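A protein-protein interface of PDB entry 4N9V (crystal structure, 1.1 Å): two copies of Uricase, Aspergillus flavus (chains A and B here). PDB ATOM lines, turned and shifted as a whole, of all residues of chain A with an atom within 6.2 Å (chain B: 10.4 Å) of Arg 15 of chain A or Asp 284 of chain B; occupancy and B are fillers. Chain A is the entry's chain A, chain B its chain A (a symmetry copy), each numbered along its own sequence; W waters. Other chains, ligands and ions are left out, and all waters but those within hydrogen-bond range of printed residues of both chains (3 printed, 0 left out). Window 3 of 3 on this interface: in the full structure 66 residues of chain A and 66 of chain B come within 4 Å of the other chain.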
ATOM      1  N   ASP A  12     -20.490   8.757 -22.834  1.00  0.00           N
ATOM      2  CA  ASP A  12     -20.949  10.043 -22.303  1.00  0.00           C
ATOM      3  C   ASP A  12     -21.869   9.797 -21.102  1.00  0.00           C
ATOM      4  O   ASP A  12     -22.458   8.712 -20.950  1.00  0.00           O
ATOM      5  CB  ASP A  12     -21.702  10.813 -23.413  1.00  0.00           C
ATOM      6  CG  ASP A  12     -21.926  12.312 -23.100  1.00  0.00           C
ATOM      7  OD1 ASP A  12     -21.439  12.826 -22.074  1.00  0.00           O
ATOM      8  OD2 ASP A  12     -22.609  12.981 -23.909  1.00  0.00           O
ATOM      9  N   ASN A  13     -22.012  10.826 -20.289  1.00  0.00           N
ATOM     10  CA  ASN A  13     -22.980  10.855 -19.213  1.00  0.00           C
ATOM     11  C   ASN A  13     -22.733   9.759 -18.184  1.00  0.00           C
ATOM     12  O   ASN A  13     -23.666   9.183 -17.631  1.00  0.00           O
ATOM     13  CB  ASN A  13     -24.401  10.828 -19.770  1.00  0.00           C
ATOM     14  CG  ASN A  13     -24.695  12.064 -20.550  1.00  0.00           C
ATOM     15  OD1 ASN A  13     -24.594  13.159 -20.010  1.00  0.00           O
ATOM     16  ND2 ASN A  13     -25.017  11.919 -21.814  1.00  0.00           N
ATOM     17  N   VAL A  14     -21.452   9.525 -17.899  1.00  0.00           N
ATOM     18  CA  VAL A  14     -21.060   8.553 -16.906  1.00  0.00           C
ATOM     19  C   VAL A  14     -21.052   9.223 -15.541  1.00  0.00           C
ATOM     20  O   VAL A  14     -20.189  10.036 -15.227  1.00  0.00           O
ATOM     21  CB  VAL A  14     -19.682   7.940 -17.202  1.00  0.00           C
ATOM     22  CG1 VAL A  14     -19.337   6.912 -16.140  1.00  0.00           C
ATOM     23  CG2 VAL A  14     -19.649   7.305 -18.579  1.00  0.00           C
ATOM     24  N   ARG A  15     -22.027   8.864 -14.712  1.00  0.00           N
ATOM     25  CA  ARG A  15     -22.126   9.411 -13.363  1.00  0.00           C
ATOM     26  C   ARG A  15     -21.158   8.673 -12.451  1.00  0.00           C
ATOM     27  O   ARG A  15     -21.077   7.447 -12.460  1.00  0.00           O
ATOM     28  CB  ARG A  15     -23.564   9.279 -12.865  1.00  0.00           C
ATOM     29  CG  ARG A  15     -24.578   9.994 -13.750  1.00  0.00           C
ATOM     30  CD  ARG A  15     -25.976   9.994 -13.150  1.00  0.00           C
ATOM     31  NE  ARG A  15     -25.982  10.754 -11.908  1.00  0.00           N
ATOM     32  CZ  ARG A  15     -26.997  10.796 -11.047  1.00  0.00           C
ATOM     33  NH1 ARG A  15     -28.105  10.097 -11.280  1.00  0.00           N
ATOM     34  NH2 ARG A  15     -26.868  11.510  -9.951  1.00  0.00           N
ATOM     35  N   VAL A  16     -20.428   9.426 -11.642  1.00  0.00           N
ATOM     36  CA  VAL A  16     -19.421   8.852 -10.755  1.00  0.00           C
ATOM     37  C   VAL A  16     -19.493   9.539  -9.405  1.00  0.00           C
ATOM     38  O   VAL A  16     -19.454  10.758  -9.338  1.00  0.00           O
ATOM     39  CB  VAL A  16     -17.984   9.023 -11.305  1.00  0.00           C
ATOM     40  CG1 VAL A  16     -16.988   8.293 -10.402  1.00  0.00           C
ATOM     41  CG2 VAL A  16     -17.876   8.547 -12.765  1.00  0.00           C
ATOM     42  N   TYR A  17     -19.591   8.750  -8.336  1.00  0.00           N
ATOM     43  CA  TYR A  17     -19.453   9.246  -6.976  1.00  0.00           C
ATOM     44  C   TYR A  17     -18.228   8.595  -6.365  1.00  0.00           C
ATOM     45  O   TYR A  17     -17.948   7.412  -6.607  1.00  0.00           O
ATOM     46  CB  TYR A  17     -20.695   8.889  -6.171  1.00  0.00           C
ATOM     47  CG  TYR A  17     -20.635   8.909  -4.665  1.00  0.00           C
ATOM     48  CD1 TYR A  17     -20.020   7.888  -3.954  1.00  0.00           C
ATOM     49  CD2 TYR A  17     -21.307   9.882  -3.952  1.00  0.00           C
ATOM     50  CE1 TYR A  17     -20.051   7.840  -2.574  1.00  0.00           C
ATOM     51  CE2 TYR A  17     -21.348   9.862  -2.570  1.00  0.00           C
ATOM     52  CZ  TYR A  17     -20.728   8.829  -1.874  1.00  0.00           C
ATOM     53  OH  TYR A  17     -20.832   8.799  -0.496  1.00  0.00           O
ATOM     54  N   GLU A  32     -18.914  14.054  -6.628  1.00  0.00           N
ATOM     55  CA  GLU A  32     -19.773  13.499  -7.648  1.00  0.00           C
ATOM     56  C   GLU A  32     -19.568  14.273  -8.936  1.00  0.00           C
ATOM     57  O   GLU A  32     -19.482  15.505  -8.927  1.00  0.00           O
ATOM     58  CB  GLU A  32     -21.245  13.495  -7.224  1.00  0.00           C
ATOM     59  CG  GLU A  32     -22.097  12.736  -8.210  1.00  0.00           C
ATOM     60  CD  GLU A  32     -23.545  12.576  -7.811  1.00  0.00           C
ATOM     61  OE1 GLU A  32     -23.854  12.550  -6.597  1.00  0.00           O
ATOM     62  OE2 GLU A  32     -24.357  12.430  -8.739  1.00  0.00           O
ATOM     63  N   MET A  33     -19.488  13.520 -10.030  1.00  0.00           N
ATOM     64  CA  MET A  33     -19.180  14.037 -11.355  1.00  0.00           C
ATOM     65  C   MET A  33     -20.082  13.395 -12.387  1.00  0.00           C
ATOM     66  O   MET A  33     -20.742  12.381 -12.124  1.00  0.00           O
ATOM     67  CB  MET A  33     -17.751  13.659 -11.755  1.00  0.00           C
ATOM     68  CG  MET A  33     -16.663  14.143 -10.840  1.00  0.00           C
ATOM     69  SD  MET A  33     -15.070  13.393 -11.282  1.00  0.00           S
ATOM     70  CE  MET A  33     -15.153  11.740 -10.592  1.00  0.00           C
ATOM     71  N   THR A  34     -20.050  13.970 -13.583  1.00  0.00           N
ATOM     72  CA  THR A  34     -20.515  13.304 -14.780  1.00  0.00           C
ATOM     73  C   THR A  34     -19.415  13.446 -15.823  1.00  0.00           C
ATOM     74  O   THR A  34     -18.920  14.548 -16.058  1.00  0.00           O
ATOM     75  CB  THR A  34     -21.827  13.892 -15.262  1.00  0.00           C
ATOM     76  OG1 THR A  34     -22.782  13.797 -14.200  1.00  0.00           O
ATOM     77  CG2 THR A  34     -22.327  13.142 -16.457  1.00  0.00           C
ATOM     78  N   VAL A  35     -19.038  12.327 -16.426  1.00  0.00           N
ATOM     79  CA  VAL A  35     -17.850  12.245 -17.262  1.00  0.00           C
ATOM     80  C   VAL A  35     -18.197  11.858 -18.672  1.00  0.00           C
ATOM     81  O   VAL A  35     -19.028  10.991 -18.909  1.00  0.00           O
ATOM     82  CB  VAL A  35     -16.861  11.195 -16.682  1.00  0.00           C
ATOM     83  CG1 VAL A  35     -15.592  11.096 -17.528  1.00  0.00           C
ATOM     84  CG2 VAL A  35     -16.532  11.529 -15.232  1.00  0.00           C
ATOM     85  N   TYR A  66     -14.379   4.184 -13.978  1.00  0.00           N
ATOM     86  CA  TYR A  66     -14.551   3.738 -12.597  1.00  0.00           C
ATOM     87  C   TYR A  66     -13.216   3.322 -11.979  1.00  0.00           C
ATOM     88  O   TYR A  66     -12.856   3.755 -10.880  1.00  0.00           O
ATOM     89  CB  TYR A  66     -15.531   2.567 -12.512  1.00  0.00           C
ATOM     90  CG  TYR A  66     -16.928   2.837 -13.024  1.00  0.00           C
ATOM     91  CD1 TYR A  66     -17.553   4.076 -12.857  1.00  0.00           C
ATOM     92  CD2 TYR A  66     -17.649   1.823 -13.618  1.00  0.00           C
ATOM     93  CE1 TYR A  66     -18.855   4.285 -13.306  1.00  0.00           C
ATOM     94  CE2 TYR A  66     -18.947   2.023 -14.054  1.00  0.00           C
ATOM     95  CZ  TYR A  66     -19.545   3.251 -13.905  1.00  0.00           C
ATOM     96  OH  TYR A  66     -20.832   3.419 -14.365  1.00  0.00           O
ATOM     97  N   HIS A 105     -20.429  18.187  -9.551  1.00  0.00           N
ATOM     98  CA  HIS A 105     -21.660  18.548  -8.871  1.00  0.00           C
ATOM     99  C   HIS A 105     -21.348  18.931  -7.441  1.00  0.00           C
ATOM    100  O   HIS A 105     -20.469  18.353  -6.817  1.00  0.00           O
ATOM    101  CB  HIS A 105     -22.625  17.364  -8.899  1.00  0.00           C
ATOM    102  CG  HIS A 105     -22.886  16.856 -10.278  1.00  0.00           C
ATOM    103  ND1 HIS A 105     -23.587  17.587 -11.218  1.00  0.00           N
ATOM    104  CD2 HIS A 105     -22.460  15.734 -10.911  1.00  0.00           C
ATOM    105  CE1 HIS A 105     -23.611  16.915 -12.357  1.00  0.00           C
ATOM    106  NE2 HIS A 105     -22.931  15.788 -12.200  1.00  0.00           N
ATOM    107  N   PRO B 254     -25.957   9.026 -30.143  1.00  0.00           N
ATOM    108  CA  PRO B 254     -25.835   8.296 -28.887  1.00  0.00           C
ATOM    109  C   PRO B 254     -26.266   6.856 -29.089  1.00  0.00           C
ATOM    110  O   PRO B 254     -27.165   6.572 -29.862  1.00  0.00           O
ATOM    111  CB  PRO B 254     -26.830   9.020 -27.974  1.00  0.00           C
ATOM    112  CG  PRO B 254     -27.876   9.550 -28.898  1.00  0.00           C
ATOM    113  CD  PRO B 254     -27.102   9.959 -30.134  1.00  0.00           C
ATOM    114  N   ASN B 255     -25.636   5.939 -28.379  1.00  0.00           N
ATOM    115  CA  ASN B 255     -26.096   4.554 -28.335  1.00  0.00           C
ATOM    116  C   ASN B 255     -26.877   4.439 -27.031  1.00  0.00           C
ATOM    117  O   ASN B 255     -26.292   4.422 -25.959  1.00  0.00           O
ATOM    118  CB  ASN B 255     -24.910   3.591 -28.390  1.00  0.00           C
ATOM    119  CG  ASN B 255     -25.320   2.168 -28.719  1.00  0.00           C
ATOM    120  OD1 ASN B 255     -26.505   1.846 -28.871  1.00  0.00           O
ATOM    121  ND2 ASN B 255     -24.327   1.303 -28.848  1.00  0.00           N
ATOM    122  N   LYS B 256     -28.206   4.452 -27.156  1.00  0.00           N
ATOM    123  CA  LYS B 256     -29.116   4.537 -26.010  1.00  0.00           C
ATOM    124  C   LYS B 256     -29.406   3.094 -25.604  1.00  0.00           C
ATOM    125  O   LYS B 256     -30.211   2.405 -26.235  1.00  0.00           O
ATOM    126  CB  LYS B 256     -30.392   5.283 -26.410  1.00  0.00           C
ATOM    127  CG  LYS B 256     -30.117   6.675 -26.940  1.00  0.00           C
ATOM    128  CD  LYS B 256     -31.375   7.352 -27.465  1.00  0.00           C
ATOM    129  CE  LYS B 256     -32.260   7.848 -26.349  1.00  0.00           C
ATOM    130  NZ  LYS B 256     -33.554   8.316 -26.866  1.00  0.00           N
ATOM    131  N   HIS B 257     -28.663   2.603 -24.620  1.00  0.00           N
ATOM    132  CA  HIS B 257     -28.586   1.171 -24.370  1.00  0.00           C
ATOM    133  C   HIS B 257     -29.866   0.610 -23.749  1.00  0.00           C
ATOM    134  O   HIS B 257     -30.491   1.240 -22.902  1.00  0.00           O
ATOM    135  CB  HIS B 257     -27.408   0.864 -23.433  1.00  0.00           C
ATOM    136  CG  HIS B 257     -26.096   1.420 -23.897  1.00  0.00           C
ATOM    137  ND1 HIS B 257     -25.460   0.993 -25.048  1.00  0.00           N
ATOM    138  CD2 HIS B 257     -25.293   2.374 -23.362  1.00  0.00           C
ATOM    139  CE1 HIS B 257     -24.334   1.674 -25.200  1.00  0.00           C
ATOM    140  NE2 HIS B 257     -24.201   2.510 -24.190  1.00  0.00           N
ATOM    141  N   TYR B 258     -30.215  -0.598 -24.178  1.00  0.00           N
ATOM    142  CA  TYR B 258     -31.299  -1.398 -23.617  1.00  0.00           C
ATOM    143  C   TYR B 258     -30.674  -2.694 -23.124  1.00  0.00           C
ATOM    144  O   TYR B 258     -30.178  -3.499 -23.916  1.00  0.00           O
ATOM    145  CB  TYR B 258     -32.374  -1.687 -24.674  1.00  0.00           C
ATOM    146  CG  TYR B 258     -33.263  -0.501 -24.959  1.00  0.00           C
ATOM    147  CD1 TYR B 258     -32.742   0.641 -25.553  1.00  0.00           C
ATOM    148  CD2 TYR B 258     -34.619  -0.510 -24.626  1.00  0.00           C
ATOM    149  CE1 TYR B 258     -33.532   1.751 -25.771  1.00  0.00           C
ATOM    150  CE2 TYR B 258     -35.426   0.597 -24.858  1.00  0.00           C
ATOM    151  CZ  TYR B 258     -34.873   1.731 -25.422  1.00  0.00           C
ATOM    152  OH  TYR B 258     -35.630   2.855 -25.656  1.00  0.00           O
ATOM    153  N   PHE B 259     -30.646  -2.867 -21.809  1.00  0.00           N
ATOM    154  CA  PHE B 259     -29.967  -3.995 -21.195  1.00  0.00           C
ATOM    155  C   PHE B 259     -30.918  -5.161 -20.975  1.00  0.00           C
ATOM    156  O   PHE B 259     -32.062  -4.982 -20.561  1.00  0.00           O
ATOM    157  CB  PHE B 259     -29.394  -3.632 -19.833  1.00  0.00           C
ATOM    158  CG  PHE B 259     -28.169  -2.744 -19.843  1.00  0.00           C
ATOM    159  CD1 PHE B 259     -27.512  -2.350 -21.012  1.00  0.00           C
ATOM    160  CD2 PHE B 259     -27.659  -2.326 -18.633  1.00  0.00           C
ATOM    161  CE1 PHE B 259     -26.367  -1.545 -20.939  1.00  0.00           C
ATOM    162  CE2 PHE B 259     -26.535  -1.534 -18.557  1.00  0.00           C
ATOM    163  CZ  PHE B 259     -25.880  -1.145 -19.714  1.00  0.00           C
ATOM    164  N   ALA B 280     -34.369  -3.481 -19.751  1.00  0.00           N
ATOM    165  CA  ALA B 280     -34.241  -2.267 -18.976  1.00  0.00           C
ATOM    166  C   ALA B 280     -33.612  -1.164 -19.840  1.00  0.00           C
ATOM    167  O   ALA B 280     -32.399  -1.189 -20.080  1.00  0.00           O
ATOM    168  CB  ALA B 280     -33.367  -2.532 -17.750  1.00  0.00           C
ATOM    169  N   PRO B 281     -34.407  -0.207 -20.332  1.00  0.00           N
ATOM    170  CA  PRO B 281     -33.812   0.946 -21.020  1.00  0.00           C
ATOM    171  C   PRO B 281     -32.939   1.718 -20.059  1.00  0.00           C
ATOM    172  O   PRO B 281     -33.374   2.003 -18.942  1.00  0.00           O
ATOM    173  CB  PRO B 281     -35.030   1.776 -21.438  1.00  0.00           C
ATOM    174  CG  PRO B 281     -36.197   0.813 -21.364  1.00  0.00           C
ATOM    175  CD  PRO B 281     -35.869  -0.070 -20.203  1.00  0.00           C
ATOM    176  N   GLN B 282     -31.723   2.058 -20.474  1.00  0.00           N
ATOM    177  CA  GLN B 282     -30.775   2.763 -19.622  1.00  0.00           C
ATOM    178  C   GLN B 282     -30.747   4.242 -19.939  1.00  0.00           C
ATOM    179  O   GLN B 282     -30.443   4.641 -21.065  1.00  0.00           O
ATOM    180  CB  GLN B 282     -29.354   2.204 -19.817  1.00  0.00           C
ATOM    181  CG  GLN B 282     -29.238   0.705 -19.580  1.00  0.00           C
ATOM    182  CD  GLN B 282     -29.539   0.329 -18.149  1.00  0.00           C
ATOM    183  OE1 GLN B 282     -28.842   0.748 -17.225  1.00  0.00           O
ATOM    184  NE2 GLN B 282     -30.581  -0.470 -17.952  1.00  0.00           N
ATOM    185  N   SER B 283     -31.018   5.075 -18.951  1.00  0.00           N
ATOM    186  CA  SER B 283     -30.993   6.508 -19.184  1.00  0.00           C
ATOM    187  C   SER B 283     -29.575   7.032 -19.374  1.00  0.00           C
ATOM    188  O   SER B 283     -29.362   7.951 -20.153  1.00  0.00           O
ATOM    189  CB  SER B 283     -31.687   7.247 -18.047  1.00  0.00           C
ATOM    190  OG  SER B 283     -33.047   6.835 -17.985  1.00  0.00           O
ATOM    191  N   ASP B 284     -28.627   6.467 -18.643  1.00  0.00           N
ATOM    192  CA  ASP B 284     -27.219   6.840 -18.714  1.00  0.00           C
ATOM    193  C   ASP B 284     -26.415   5.686 -18.147  1.00  0.00           C
ATOM    194  O   ASP B 284     -26.938   4.857 -17.410  1.00  0.00           O
ATOM    195  CB  ASP B 284     -26.942   8.134 -17.930  1.00  0.00           C
ATOM    196  CG  ASP B 284     -27.417   8.057 -16.492  1.00  0.00           C
ATOM    197  OD1 ASP B 284     -26.657   7.526 -15.652  1.00  0.00           O
ATOM    198  OD2 ASP B 284     -28.534   8.552 -16.214  1.00  0.00           O
ATOM    199  N   PRO B 285     -25.143   5.609 -18.521  1.00  0.00           N
ATOM    200  CA  PRO B 285     -24.522   6.456 -19.533  1.00  0.00           C
ATOM    201  C   PRO B 285     -24.921   5.964 -20.910  1.00  0.00           C
ATOM    202  O   PRO B 285     -25.691   5.003 -21.059  1.00  0.00           O
ATOM    203  CB  PRO B 285     -23.032   6.238 -19.283  1.00  0.00           C
ATOM    204  CG  PRO B 285     -22.953   4.837 -18.835  1.00  0.00           C
ATOM    205  CD  PRO B 285     -24.208   4.593 -18.013  1.00  0.00           C
ATOM    206  N   ASN B 286     -24.384   6.620 -21.930  1.00  0.00           N
ATOM    207  CA  ASN B 286     -24.672   6.256 -23.306  1.00  0.00           C
ATOM    208  C   ASN B 286     -23.395   6.321 -24.111  1.00  0.00           C
ATOM    209  O   ASN B 286     -22.583   7.216 -23.935  1.00  0.00           O
ATOM    210  CB  ASN B 286     -25.729   7.178 -23.945  1.00  0.00           C
ATOM    211  CG  ASN B 286     -25.317   8.646 -23.932  1.00  0.00           C
ATOM    212  OD1 ASN B 286     -25.484   9.331 -22.927  1.00  0.00           O
ATOM    213  ND2 ASN B 286     -24.818   9.141 -25.052  1.00  0.00           N
ATOM    214  N   GLY B 287     -23.234   5.401 -25.045  1.00  0.00           N
ATOM    215  CA  GLY B 287     -22.198   5.585 -26.048  1.00  0.00           C
ATOM    216  C   GLY B 287     -22.471   6.852 -26.837  1.00  0.00           C
ATOM    217  O   GLY B 287     -23.621   7.268 -26.979  1.00  0.00           O
HETATM  218  O   HOH W   1     -27.406   9.618 -21.042  1.00  0.00           O
HETATM  219  O   HOH W   2     -24.304  11.970 -25.357  1.00  0.00           O
HETATM  220  O   HOH W   3     -23.976   6.876 -15.363  1.00  0.00           O
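No position is printed for both chains.
Of the printed residues of chain B, Arg 15 of chain A touches Asp 284. Asp 284 of chain B touches just these residues of chain A: Asn 13 and Arg 15. Val 16 of chain A touches none of the printed residues of chain B. Of the printed residues of chain B, Asp 12 of chain A touches Pro 285 and Asn 286. Printed residues of chain A within 4 Å of Asn 286 of chain B: Asp 12 (2.8 Å) and Asn 13 (2.9 Å). Of the printed residues of chain B, Val 14 of chain A touches Pro 285 (3.6 Å). Gly 287 of chain B touches none of the printed residues of chain A. Pro 254 of chain B touches none of the printed residues of chain A. The nearest printed residue of chain B that does not touch Arg 15 of chain A is Pro 285 of chain B (5.4 Å).
The side-chain amide nitrogen (ND2) of Asn 13 of chain A lies within hydrogen-bond range of the side-chain amide oxygen (OD1) of Asn 286 of chain B. N of Asp 12 of chain A is in hydrogen-bond range of O of Asn 286 of chain B.
O of Val 35 of chain A sits at hydrogen-bond distance from N of Asn 13 of chain A, 3.3 Å away. The backbone carbonyl oxygen of Val 14 of chain A is in hydrogen-bond range of the backbone NH of Val 35 of chain A, at 2.8 Å. NH2 of Arg 15 of chain A is in salt-bridge range of OE2 of Glu 32 of chain A (2.9 Å). OD2 of Asp 12 of chain A sits at hydrogen-bond distance from ND2 of Asn 13 of chain A (3.4 Å).
Water W2 bridges OD2 of Asp 12 of chain A (2.4 Å) and ND2 of Asn 286 of chain B (2.9 Å). Water W1 lies within hydrogen-bond range of OD1 of Asn 286 of chain B (2.7 Å), O of Ser 283 of chain B (2.7 Å) and ND2 of Asn 13 of chain A (3.4 Å). Water W3 lies within hydrogen-bond range of the side-chain carboxylate of Asp 284 of chain B (2.8 Å), the backbone NH of Arg 15 of chain A (2.9 Å) and the backbone carbonyl oxygen of Asn 13 of chain A (3.2 Å).
Of the 14 printed residues of chain B, 3 touch a printed residue of chain A. Printed residues of chain B that touch a printed residue of chain A: Asp 284, Pro 285 and Asn 286. Hydrophobic or aromatic side chains of chain B that line the printed part of chain A: Pro 285. Among the printed residues, no Asp or Glu carboxylate lies within 4 Å of a Lys or Arg side-chain nitrogen of the other chain.
Among the printed residues, merely in contact across the chains: Asp 12 of chain A with Pro 285 of chain B, Asn 13 of chain A with Asp 284 of chain B, Asn 13 of chain A with Pro 285 of chain B, Val 14 of chain A with Pro 285 of chain B and Arg 15 of chain A with Asp 284 of chain B.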
